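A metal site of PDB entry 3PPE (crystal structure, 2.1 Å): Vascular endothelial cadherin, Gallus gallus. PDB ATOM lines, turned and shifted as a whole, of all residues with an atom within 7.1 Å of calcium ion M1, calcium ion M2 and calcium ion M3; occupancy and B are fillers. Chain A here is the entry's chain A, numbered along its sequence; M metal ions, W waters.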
ATOM      1  N   GLU A  11     -22.056 -23.725  13.103  1.00  0.00           N
ATOM      2  CA  GLU A  11     -22.172 -23.968  14.536  1.00  0.00           C
ATOM      3  C   GLU A  11     -22.995 -22.892  15.192  1.00  0.00           C
ATOM      4  O   GLU A  11     -23.142 -21.790  14.646  1.00  0.00           O
ATOM      5  CB  GLU A  11     -20.786 -24.036  15.208  1.00  0.00           C
ATOM      6  CG  GLU A  11     -20.031 -22.709  15.092  1.00  0.00           C
ATOM      7  CD  GLU A  11     -18.868 -22.577  16.074  1.00  0.00           C
ATOM      8  OE1 GLU A  11     -18.912 -23.196  17.164  1.00  0.00           O
ATOM      9  OE2 GLU A  11     -17.917 -21.848  15.737  1.00  0.00           O
ATOM     10  N   GLU A  12     -23.531 -23.221  16.373  1.00  0.00           N
ATOM     11  CA  GLU A  12     -24.168 -22.230  17.293  1.00  0.00           C
ATOM     12  C   GLU A  12     -25.428 -21.547  16.702  1.00  0.00           C
ATOM     13  O   GLU A  12     -25.720 -20.391  16.986  1.00  0.00           O
ATOM     14  CB  GLU A  12     -23.150 -21.166  17.749  1.00  0.00           C
ATOM     15  CG  GLU A  12     -21.800 -21.714  18.236  1.00  0.00           C
ATOM     16  CD  GLU A  12     -21.835 -22.486  19.546  1.00  0.00           C
ATOM     17  OE1 GLU A  12     -20.741 -22.830  20.034  1.00  0.00           O
ATOM     18  OE2 GLU A  12     -22.904 -22.790  20.122  1.00  0.00           O
ATOM     19  N   ARG A  60     -28.025 -27.899  18.691  1.00  0.00           N
ATOM     20  CA  ARG A  60     -27.087 -26.849  18.349  1.00  0.00           C
ATOM     21  C   ARG A  60     -25.678 -27.426  18.472  1.00  0.00           C
ATOM     22  O   ARG A  60     -25.398 -28.217  19.397  1.00  0.00           O
ATOM     23  CB  ARG A  60     -27.226 -25.665  19.292  1.00  0.00           C
ATOM     24  CG  ARG A  60     -28.485 -24.873  19.071  1.00  0.00           C
ATOM     25  CD  ARG A  60     -28.505 -23.684  20.015  1.00  0.00           C
ATOM     26  NE  ARG A  60     -27.280 -22.899  19.845  1.00  0.00           N
ATOM     27  CZ  ARG A  60     -26.258 -22.857  20.698  1.00  0.00           C
ATOM     28  NH1 ARG A  60     -26.270 -23.538  21.848  1.00  0.00           N
ATOM     29  NH2 ARG A  60     -25.218 -22.104  20.403  1.00  0.00           N
ATOM     30  N   LEU A  61     -24.810 -27.038  17.557  1.00  0.00           N
ATOM     31  CA  LEU A  61     -23.480 -27.588  17.450  1.00  0.00           C
ATOM     32  C   LEU A  61     -22.366 -26.565  17.846  1.00  0.00           C
ATOM     33  O   LEU A  61     -22.478 -25.383  17.593  1.00  0.00           O
ATOM     34  CB  LEU A  61     -23.245 -28.075  16.005  1.00  0.00           C
ATOM     35  CG  LEU A  61     -24.250 -29.107  15.470  1.00  0.00           C
ATOM     36  CD1 LEU A  61     -24.080 -29.293  13.961  1.00  0.00           C
ATOM     37  CD2 LEU A  61     -24.132 -30.423  16.252  1.00  0.00           C
ATOM     38  N   ASP A  62     -21.299 -27.070  18.426  1.00  0.00           N
ATOM     39  CA  ASP A  62     -20.162 -26.227  18.766  1.00  0.00           C
ATOM     40  C   ASP A  62     -18.974 -26.800  18.051  1.00  0.00           C
ATOM     41  O   ASP A  62     -18.512 -27.862  18.408  1.00  0.00           O
ATOM     42  CB  ASP A  62     -19.953 -26.291  20.285  1.00  0.00           C
ATOM     43  CG  ASP A  62     -18.796 -25.427  20.761  1.00  0.00           C
ATOM     44  OD1 ASP A  62     -18.161 -24.684  19.967  1.00  0.00           O
ATOM     45  OD2 ASP A  62     -18.525 -25.515  21.962  1.00  0.00           O
ATOM     46  N   ARG A  63     -18.494 -26.100  17.031  1.00  0.00           N
ATOM     47  CA  ARG A  63     -17.280 -26.548  16.300  1.00  0.00           C
ATOM     48  C   ARG A  63     -16.068 -26.764  17.241  1.00  0.00           C
ATOM     49  O   ARG A  63     -15.225 -27.631  16.997  1.00  0.00           O
ATOM     50  CB  ARG A  63     -16.928 -25.569  15.169  1.00  0.00           C
ATOM     51  CG  ARG A  63     -15.935 -26.117  14.157  1.00  0.00           C
ATOM     52  CD  ARG A  63     -15.137 -24.955  13.531  1.00  0.00           C
ATOM     53  NE  ARG A  63     -14.272 -24.313  14.559  1.00  0.00           N
ATOM     54  CZ  ARG A  63     -13.068 -24.773  14.903  1.00  0.00           C
ATOM     55  NH1 ARG A  63     -12.588 -25.846  14.318  1.00  0.00           N
ATOM     56  NH2 ARG A  63     -12.364 -24.189  15.870  1.00  0.00           N
ATOM     57  N   GLU A  64     -16.005 -25.990  18.310  1.00  0.00           N
ATOM     58  CA  GLU A  64     -14.882 -26.113  19.237  1.00  0.00           C
ATOM     59  C   GLU A  64     -14.940 -27.370  20.109  1.00  0.00           C
ATOM     60  O   GLU A  64     -13.941 -27.754  20.720  1.00  0.00           O
ATOM     61  CB  GLU A  64     -14.745 -24.849  20.104  1.00  0.00           C
ATOM     62  CG  GLU A  64     -14.102 -23.671  19.363  1.00  0.00           C
ATOM     63  CD  GLU A  64     -14.994 -23.011  18.339  1.00  0.00           C
ATOM     64  OE1 GLU A  64     -16.145 -22.610  18.648  1.00  0.00           O
ATOM     65  OE2 GLU A  64     -14.535 -22.856  17.187  1.00  0.00           O
ATOM     66  N   LYS A  65     -16.106 -28.028  20.148  1.00  0.00           N
ATOM     67  CA  LYS A  65     -16.259 -29.348  20.787  1.00  0.00           C
ATOM     68  C   LYS A  65     -15.973 -30.465  19.770  1.00  0.00           C
ATOM     69  O   LYS A  65     -15.186 -31.377  20.030  1.00  0.00           O
ATOM     70  CB  LYS A  65     -17.705 -29.487  21.190  1.00  0.00           C
ATOM     71  CG  LYS A  65     -17.968 -29.854  22.614  1.00  0.00           C
ATOM     72  CD  LYS A  65     -17.785 -28.630  23.523  1.00  0.00           C
ATOM     73  CE  LYS A  65     -18.711 -28.700  24.742  1.00  0.00           C
ATOM     74  NZ  LYS A  65     -18.015 -28.196  25.966  1.00  0.00           N
ATOM     75  N   SER A  95     -19.229 -25.571  10.278  1.00  0.00           N
ATOM     76  CA  SER A  95     -18.625 -24.325   9.802  1.00  0.00           C
ATOM     77  C   SER A  95     -18.451 -23.375  10.979  1.00  0.00           C
ATOM     78  O   SER A  95     -19.363 -23.171  11.750  1.00  0.00           O
ATOM     79  CB  SER A  95     -19.522 -23.647   8.753  1.00  0.00           C
ATOM     80  OG  SER A  95     -19.847 -24.586   7.737  1.00  0.00           O
ATOM     81  N   ASP A  96     -17.273 -22.790  11.083  1.00  0.00           N
ATOM     82  CA  ASP A  96     -16.874 -21.945  12.206  1.00  0.00           C
ATOM     83  C   ASP A  96     -17.549 -20.576  12.223  1.00  0.00           C
ATOM     84  O   ASP A  96     -17.570 -19.889  11.211  1.00  0.00           O
ATOM     85  CB  ASP A  96     -15.348 -21.724  12.121  1.00  0.00           C
ATOM     86  CG  ASP A  96     -14.771 -21.135  13.387  1.00  0.00           C
ATOM     87  OD1 ASP A  96     -13.965 -20.172  13.285  1.00  0.00           O
ATOM     88  OD2 ASP A  96     -15.092 -21.608  14.503  1.00  0.00           O
ATOM     89  N   ILE A  97     -18.039 -20.154  13.373  1.00  0.00           N
ATOM     90  CA  ILE A  97     -18.302 -18.742  13.571  1.00  0.00           C
ATOM     91  C   ILE A  97     -17.224 -18.182  14.510  1.00  0.00           C
ATOM     92  O   ILE A  97     -16.587 -18.924  15.277  1.00  0.00           O
ATOM     93  CB  ILE A  97     -19.767 -18.444  14.094  1.00  0.00           C
ATOM     94  CG1 ILE A  97     -19.995 -18.889  15.549  1.00  0.00           C
ATOM     95  CG2 ILE A  97     -20.859 -19.026  13.089  1.00  0.00           C
ATOM     96  CD1 ILE A  97     -21.192 -18.161  16.242  1.00  0.00           C
ATOM     97  N   ASN A  98     -17.034 -16.872  14.456  1.00  0.00           N
ATOM     98  CA  ASN A  98     -16.115 -16.216  15.368  1.00  0.00           C
ATOM     99  C   ASN A  98     -16.758 -16.042  16.753  1.00  0.00           C
ATOM    100  O   ASN A  98     -17.400 -15.048  17.034  1.00  0.00           O
ATOM    101  CB  ASN A  98     -15.614 -14.879  14.804  1.00  0.00           C
ATOM    102  CG  ASN A  98     -14.382 -14.404  15.554  1.00  0.00           C
ATOM    103  OD1 ASN A  98     -13.508 -15.239  15.892  1.00  0.00           O
ATOM    104  ND2 ASN A  98     -14.310 -13.145  15.887  1.00  0.00           N
ATOM    105  N   ASP A  99     -16.613 -17.032  17.615  1.00  0.00           N
ATOM    106  CA  ASP A  99     -17.246 -16.964  18.915  1.00  0.00           C
ATOM    107  C   ASP A  99     -16.280 -17.132  20.100  1.00  0.00           C
ATOM    108  O   ASP A  99     -16.704 -17.298  21.222  1.00  0.00           O
ATOM    109  CB  ASP A  99     -18.452 -17.925  19.006  1.00  0.00           C
ATOM    110  CG  ASP A  99     -18.104 -19.392  18.758  1.00  0.00           C
ATOM    111  OD1 ASP A  99     -17.089 -19.736  18.099  1.00  0.00           O
ATOM    112  OD2 ASP A  99     -18.917 -20.261  19.228  1.00  0.00           O
ATOM    113  N   ASN A 100     -14.969 -17.090  19.814  1.00  0.00           N
ATOM    114  CA  ASN A 100     -13.951 -17.135  20.834  1.00  0.00           C
ATOM    115  C   ASN A 100     -12.983 -15.969  20.722  1.00  0.00           C
ATOM    116  O   ASN A 100     -12.594 -15.541  19.619  1.00  0.00           O
ATOM    117  CB  ASN A 100     -13.173 -18.481  20.820  1.00  0.00           C
ATOM    118  CG  ASN A 100     -14.066 -19.685  21.122  1.00  0.00           C
ATOM    119  OD1 ASN A 100     -14.707 -20.225  20.224  1.00  0.00           O
ATOM    120  ND2 ASN A 100     -14.156 -20.067  22.386  1.00  0.00           N
ATOM    121  N   ALA A 101     -12.601 -15.434  21.869  1.00  0.00           N
ATOM    122  CA  ALA A 101     -11.578 -14.390  21.901  1.00  0.00           C
ATOM    123  C   ALA A 101     -10.212 -15.059  22.207  1.00  0.00           C
ATOM    124  O   ALA A 101     -10.159 -16.194  22.702  1.00  0.00           O
ATOM    125  CB  ALA A 101     -11.933 -13.324  22.953  1.00  0.00           C
ATOM    126  N   PRO A 102      -9.103 -14.402  21.835  1.00  0.00           N
ATOM    127  CA  PRO A 102      -7.794 -14.977  22.245  1.00  0.00           C
ATOM    128  C   PRO A 102      -7.639 -14.906  23.754  1.00  0.00           C
ATOM    129  O   PRO A 102      -8.075 -13.907  24.403  1.00  0.00           O
ATOM    130  CB  PRO A 102      -6.767 -14.066  21.539  1.00  0.00           C
ATOM    131  CG  PRO A 102      -7.620 -13.365  20.423  1.00  0.00           C
ATOM    132  CD  PRO A 102      -8.952 -13.157  21.068  1.00  0.00           C
ATOM    133  N   ASP A 130      -6.491 -18.458  20.268  1.00  0.00           N
ATOM    134  CA  ASP A 130      -7.893 -18.220  19.951  1.00  0.00           C
ATOM    135  C   ASP A 130      -8.419 -19.556  19.451  1.00  0.00           C
ATOM    136  O   ASP A 130      -7.873 -20.104  18.499  1.00  0.00           O
ATOM    137  CB  ASP A 130      -7.978 -17.183  18.854  1.00  0.00           C
ATOM    138  CG  ASP A 130      -9.394 -16.751  18.565  1.00  0.00           C
ATOM    139  OD1 ASP A 130     -10.290 -17.581  18.272  1.00  0.00           O
ATOM    140  OD2 ASP A 130      -9.599 -15.543  18.540  1.00  0.00           O
ATOM    141  N   ALA A 131      -9.490 -20.041  20.092  1.00  0.00           N
ATOM    142  CA  ALA A 131     -10.016 -21.385  19.849  1.00  0.00           C
ATOM    143  C   ALA A 131     -10.804 -21.544  18.528  1.00  0.00           C
ATOM    144  O   ALA A 131     -11.176 -22.661  18.143  1.00  0.00           O
ATOM    145  CB  ALA A 131     -10.885 -21.780  21.023  1.00  0.00           C
ATOM    146  N   ASP A 132     -11.066 -20.444  17.831  1.00  0.00           N
ATOM    147  CA  ASP A 132     -11.742 -20.498  16.536  1.00  0.00           C
ATOM    148  C   ASP A 132     -10.860 -21.155  15.468  1.00  0.00           C
ATOM    149  O   ASP A 132      -9.688 -21.484  15.720  1.00  0.00           O
ATOM    150  CB  ASP A 132     -12.279 -19.117  16.104  1.00  0.00           C
ATOM    151  CG  ASP A 132     -13.328 -18.618  17.058  1.00  0.00           C
ATOM    152  OD1 ASP A 132     -14.220 -19.403  17.381  1.00  0.00           O
ATOM    153  OD2 ASP A 132     -13.272 -17.443  17.531  1.00  0.00           O
ATOM    154  N   ASP A 133     -11.426 -21.334  14.287  1.00  0.00           N
ATOM    155  CA  ASP A 133     -10.745 -22.058  13.211  1.00  0.00           C
ATOM    156  C   ASP A 133      -9.734 -21.164  12.499  1.00  0.00           C
ATOM    157  O   ASP A 133     -10.096 -20.125  11.946  1.00  0.00           O
ATOM    158  CB  ASP A 133     -11.759 -22.606  12.213  1.00  0.00           C
ATOM    159  CG  ASP A 133     -11.129 -23.555  11.205  1.00  0.00           C
ATOM    160  OD1 ASP A 133     -11.869 -24.318  10.562  1.00  0.00           O
ATOM    161  OD2 ASP A 133      -9.891 -23.527  11.057  1.00  0.00           O
ATOM    162  N   GLY A 138      -9.675 -14.893   9.514  1.00  0.00           N
ATOM    163  CA  GLY A 138      -9.317 -13.961  10.558  1.00  0.00           C
ATOM    164  C   GLY A 138      -9.780 -14.428  11.930  1.00  0.00           C
ATOM    165  O   GLY A 138      -9.475 -13.793  12.945  1.00  0.00           O
ATOM    166  N   HIS A 139     -10.524 -15.523  11.961  1.00  0.00           N
ATOM    167  CA  HIS A 139     -11.270 -15.912  13.152  1.00  0.00           C
ATOM    168  C   HIS A 139     -10.340 -16.196  14.318  1.00  0.00           C
ATOM    169  O   HIS A 139     -10.691 -15.945  15.474  1.00  0.00           O
ATOM    170  CB  HIS A 139     -12.134 -17.147  12.858  1.00  0.00           C
ATOM    171  CG  HIS A 139     -13.393 -16.836  12.109  1.00  0.00           C
ATOM    172  ND1 HIS A 139     -14.449 -17.717  12.029  1.00  0.00           N
ATOM    173  CD2 HIS A 139     -13.773 -15.733  11.404  1.00  0.00           C
ATOM    174  CE1 HIS A 139     -15.415 -17.186  11.314  1.00  0.00           C
ATOM    175  NE2 HIS A 139     -15.030 -15.982  10.920  1.00  0.00           N
ATOM    176  N   ALA A 140      -9.149 -16.712  14.020  1.00  0.00           N
ATOM    177  CA  ALA A 140      -8.178 -17.036  15.044  1.00  0.00           C
ATOM    178  C   ALA A 140      -6.925 -16.180  14.823  1.00  0.00           C
ATOM    179  O   ALA A 140      -5.814 -16.556  15.227  1.00  0.00           O
ATOM    180  CB  ALA A 140      -7.854 -18.487  14.962  1.00  0.00           C
ATOM    181  N   THR A 141      -7.085 -15.045  14.180  1.00  0.00           N
ATOM    182  CA  THR A 141      -5.988 -14.139  13.972  1.00  0.00           C
ATOM    183  C   THR A 141      -5.857 -13.280  15.248  1.00  0.00           C
ATOM    184  O   THR A 141      -6.774 -12.533  15.572  1.00  0.00           O
ATOM    185  CB  THR A 141      -6.271 -13.198  12.784  1.00  0.00           C
ATOM    186  OG1 THR A 141      -6.369 -13.953  11.572  1.00  0.00           O
ATOM    187  CG2 THR A 141      -5.123 -12.203  12.602  1.00  0.00           C
ATOM    188  N   ASP A 184      -8.764 -10.717  18.556  1.00  0.00           N
ATOM    189  CA  ASP A 184      -8.750 -11.273  17.208  1.00  0.00           C
ATOM    190  C   ASP A 184      -9.178 -10.233  16.182  1.00  0.00           C
ATOM    191  O   ASP A 184      -9.773  -9.212  16.526  1.00  0.00           O
ATOM    192  CB  ASP A 184      -9.663 -12.498  17.123  1.00  0.00           C
ATOM    193  CG  ASP A 184     -11.127 -12.136  17.106  1.00  0.00           C
ATOM    194  OD1 ASP A 184     -11.973 -13.012  17.380  1.00  0.00           O
ATOM    195  OD2 ASP A 184     -11.443 -10.960  16.819  1.00  0.00           O
ATOM    196  N   ALA A 185      -8.859 -10.490  14.915  1.00  0.00           N
ATOM    197  CA  ALA A 185      -8.848  -9.446  13.901  1.00  0.00           C
ATOM    198  C   ALA A 185     -10.252  -8.909  13.644  1.00  0.00           C
ATOM    199  O   ALA A 185     -10.424  -7.867  13.022  1.00  0.00           O
ATOM    200  CB  ALA A 185      -8.241  -9.970  12.609  1.00  0.00           C
ATOM    201  N   LEU A 186     -11.256  -9.632  14.143  1.00  0.00           N
ATOM    202  CA  LEU A 186     -12.641  -9.211  14.003  1.00  0.00           C
ATOM    203  C   LEU A 186     -13.123  -8.451  15.224  1.00  0.00           C
ATOM    204  O   LEU A 186     -14.243  -7.946  15.261  1.00  0.00           O
ATOM    205  CB  LEU A 186     -13.543 -10.420  13.739  1.00  0.00           C
ATOM    206  CG  LEU A 186     -13.465 -11.042  12.342  1.00  0.00           C
ATOM    207  CD1 LEU A 186     -12.222 -11.902  12.216  1.00  0.00           C
ATOM    208  CD2 LEU A 186     -14.721 -11.856  12.045  1.00  0.00           C
ATOM    209  N   LEU A 188     -12.865  -9.406  18.627  1.00  0.00           N
ATOM    210  CA  LEU A 188     -13.374 -10.157  19.774  1.00  0.00           C
ATOM    211  C   LEU A 188     -12.395 -10.117  20.937  1.00  0.00           C
ATOM    212  O   LEU A 188     -11.295 -10.651  20.855  1.00  0.00           O
ATOM    213  CB  LEU A 188     -13.656 -11.605  19.371  1.00  0.00           C
ATOM    214  CG  LEU A 188     -15.006 -12.185  19.822  1.00  0.00           C
ATOM    215  CD1 LEU A 188     -16.146 -11.243  19.447  1.00  0.00           C
ATOM    216  CD2 LEU A 188     -15.227 -13.568  19.229  1.00  0.00           C
HETATM  217 CA    CA M   1     -15.960 -20.876  16.539  1.00  0.00          CA
HETATM  218 CA    CA M   2     -18.347 -22.511  19.343  1.00  0.00          CA
HETATM  219 CA    CA M   3     -11.770 -15.622  17.467  1.00  0.00          CA
HETATM  220  O   HOH W   1     -17.340 -21.706  21.448  1.00  0.00           O
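The side-chain amide oxygen (OD1) of Asn 100 sits close to the side-chain carboxylate (OD1) of Asp 99, at 3.2 Å. The side-chain carboxylate of Glu 64 sits close to the side-chain amide oxygen of Asn 100 (3.2 Å). The side-chain carboxylate (OE1) of Glu 11 lies close to the backbone NH (N) of Arg 63 (2.9 Å). N of Glu 11 lies within hydrogen-bond range of O of Ser 95 (3.1 Å). The side-chain carboxylate of Asp 96 sits at hydrogen-bond distance from the backbone NH of Asp 133 (3.0 Å). N of Glu 12 is in hydrogen-bond range of O of Leu 61. The side-chain carboxylate (OE2) of Glu 12 lies within salt-bridge range of the guanidinium group (NH2) of Arg 60 (2.4 Å). OD2 of Asp 184 lies within hydrogen-bond range of N of Leu 188 (2.8 Å).
Seven residues have an atom within 4 Å of calcium ion M1: Glu 11, Glu 64, Asp 96, Ile 97, Asp 99, Asn 100 and Asp 132.
Of the 28 residues printed, 5 come within 4 Å of calcium ion M2. Along chain A the residues within 4 Å of calcium ion M2 span positions 11 to 99.
Of the 28 residues printed, 6 come within 4 Å of calcium ion M3. The nearest printed residue that does not touch calcium ion M3 is Leu 188 (4.4 Å).
Calcium ion M1 is bound by OD1 of Asp 99 (2.2 Å), OE2 of Glu 11 (2.3 Å), OD2 of Asp 96 (2.3 Å), O of Ile 97 (2.4 Å), OD1 of Asp 132 (2.4 Å), OE2 of Glu 64 (2.5 Å) and OE1 of Glu 64 (2.7 Å). Calcium ion M1 has seven donor atoms within binding distance.
Calcium ion M2 is bound by OD1 of Asp 62 (2.3 Å), OE1 of Glu 64 (2.3 Å), OD2 of Asp 99 (2.3 Å), OE1 of Glu 11 (2.4 Å), water W1 (2.5 Å) and OE1 of Glu 12 (2.5 Å).
Calcium ion M3 is bound by the backbone carbonyl oxygen (O) of His 139 (2.3 Å), the backbone carbonyl oxygen (O) of Asn 100 (2.3 Å), the side-chain carboxylate (OD2) of Asp 132 (2.4 Å), the side-chain amide oxygen (OD1) of Asn 98 (2.4 Å), the side-chain carboxylate (OD2) of Asp 130 (2.4 Å), the side-chain carboxylate (OD1) of Asp 130 (2.6 Å) and the side-chain carboxylate (OD1) of Asp 184 (2.6 Å).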
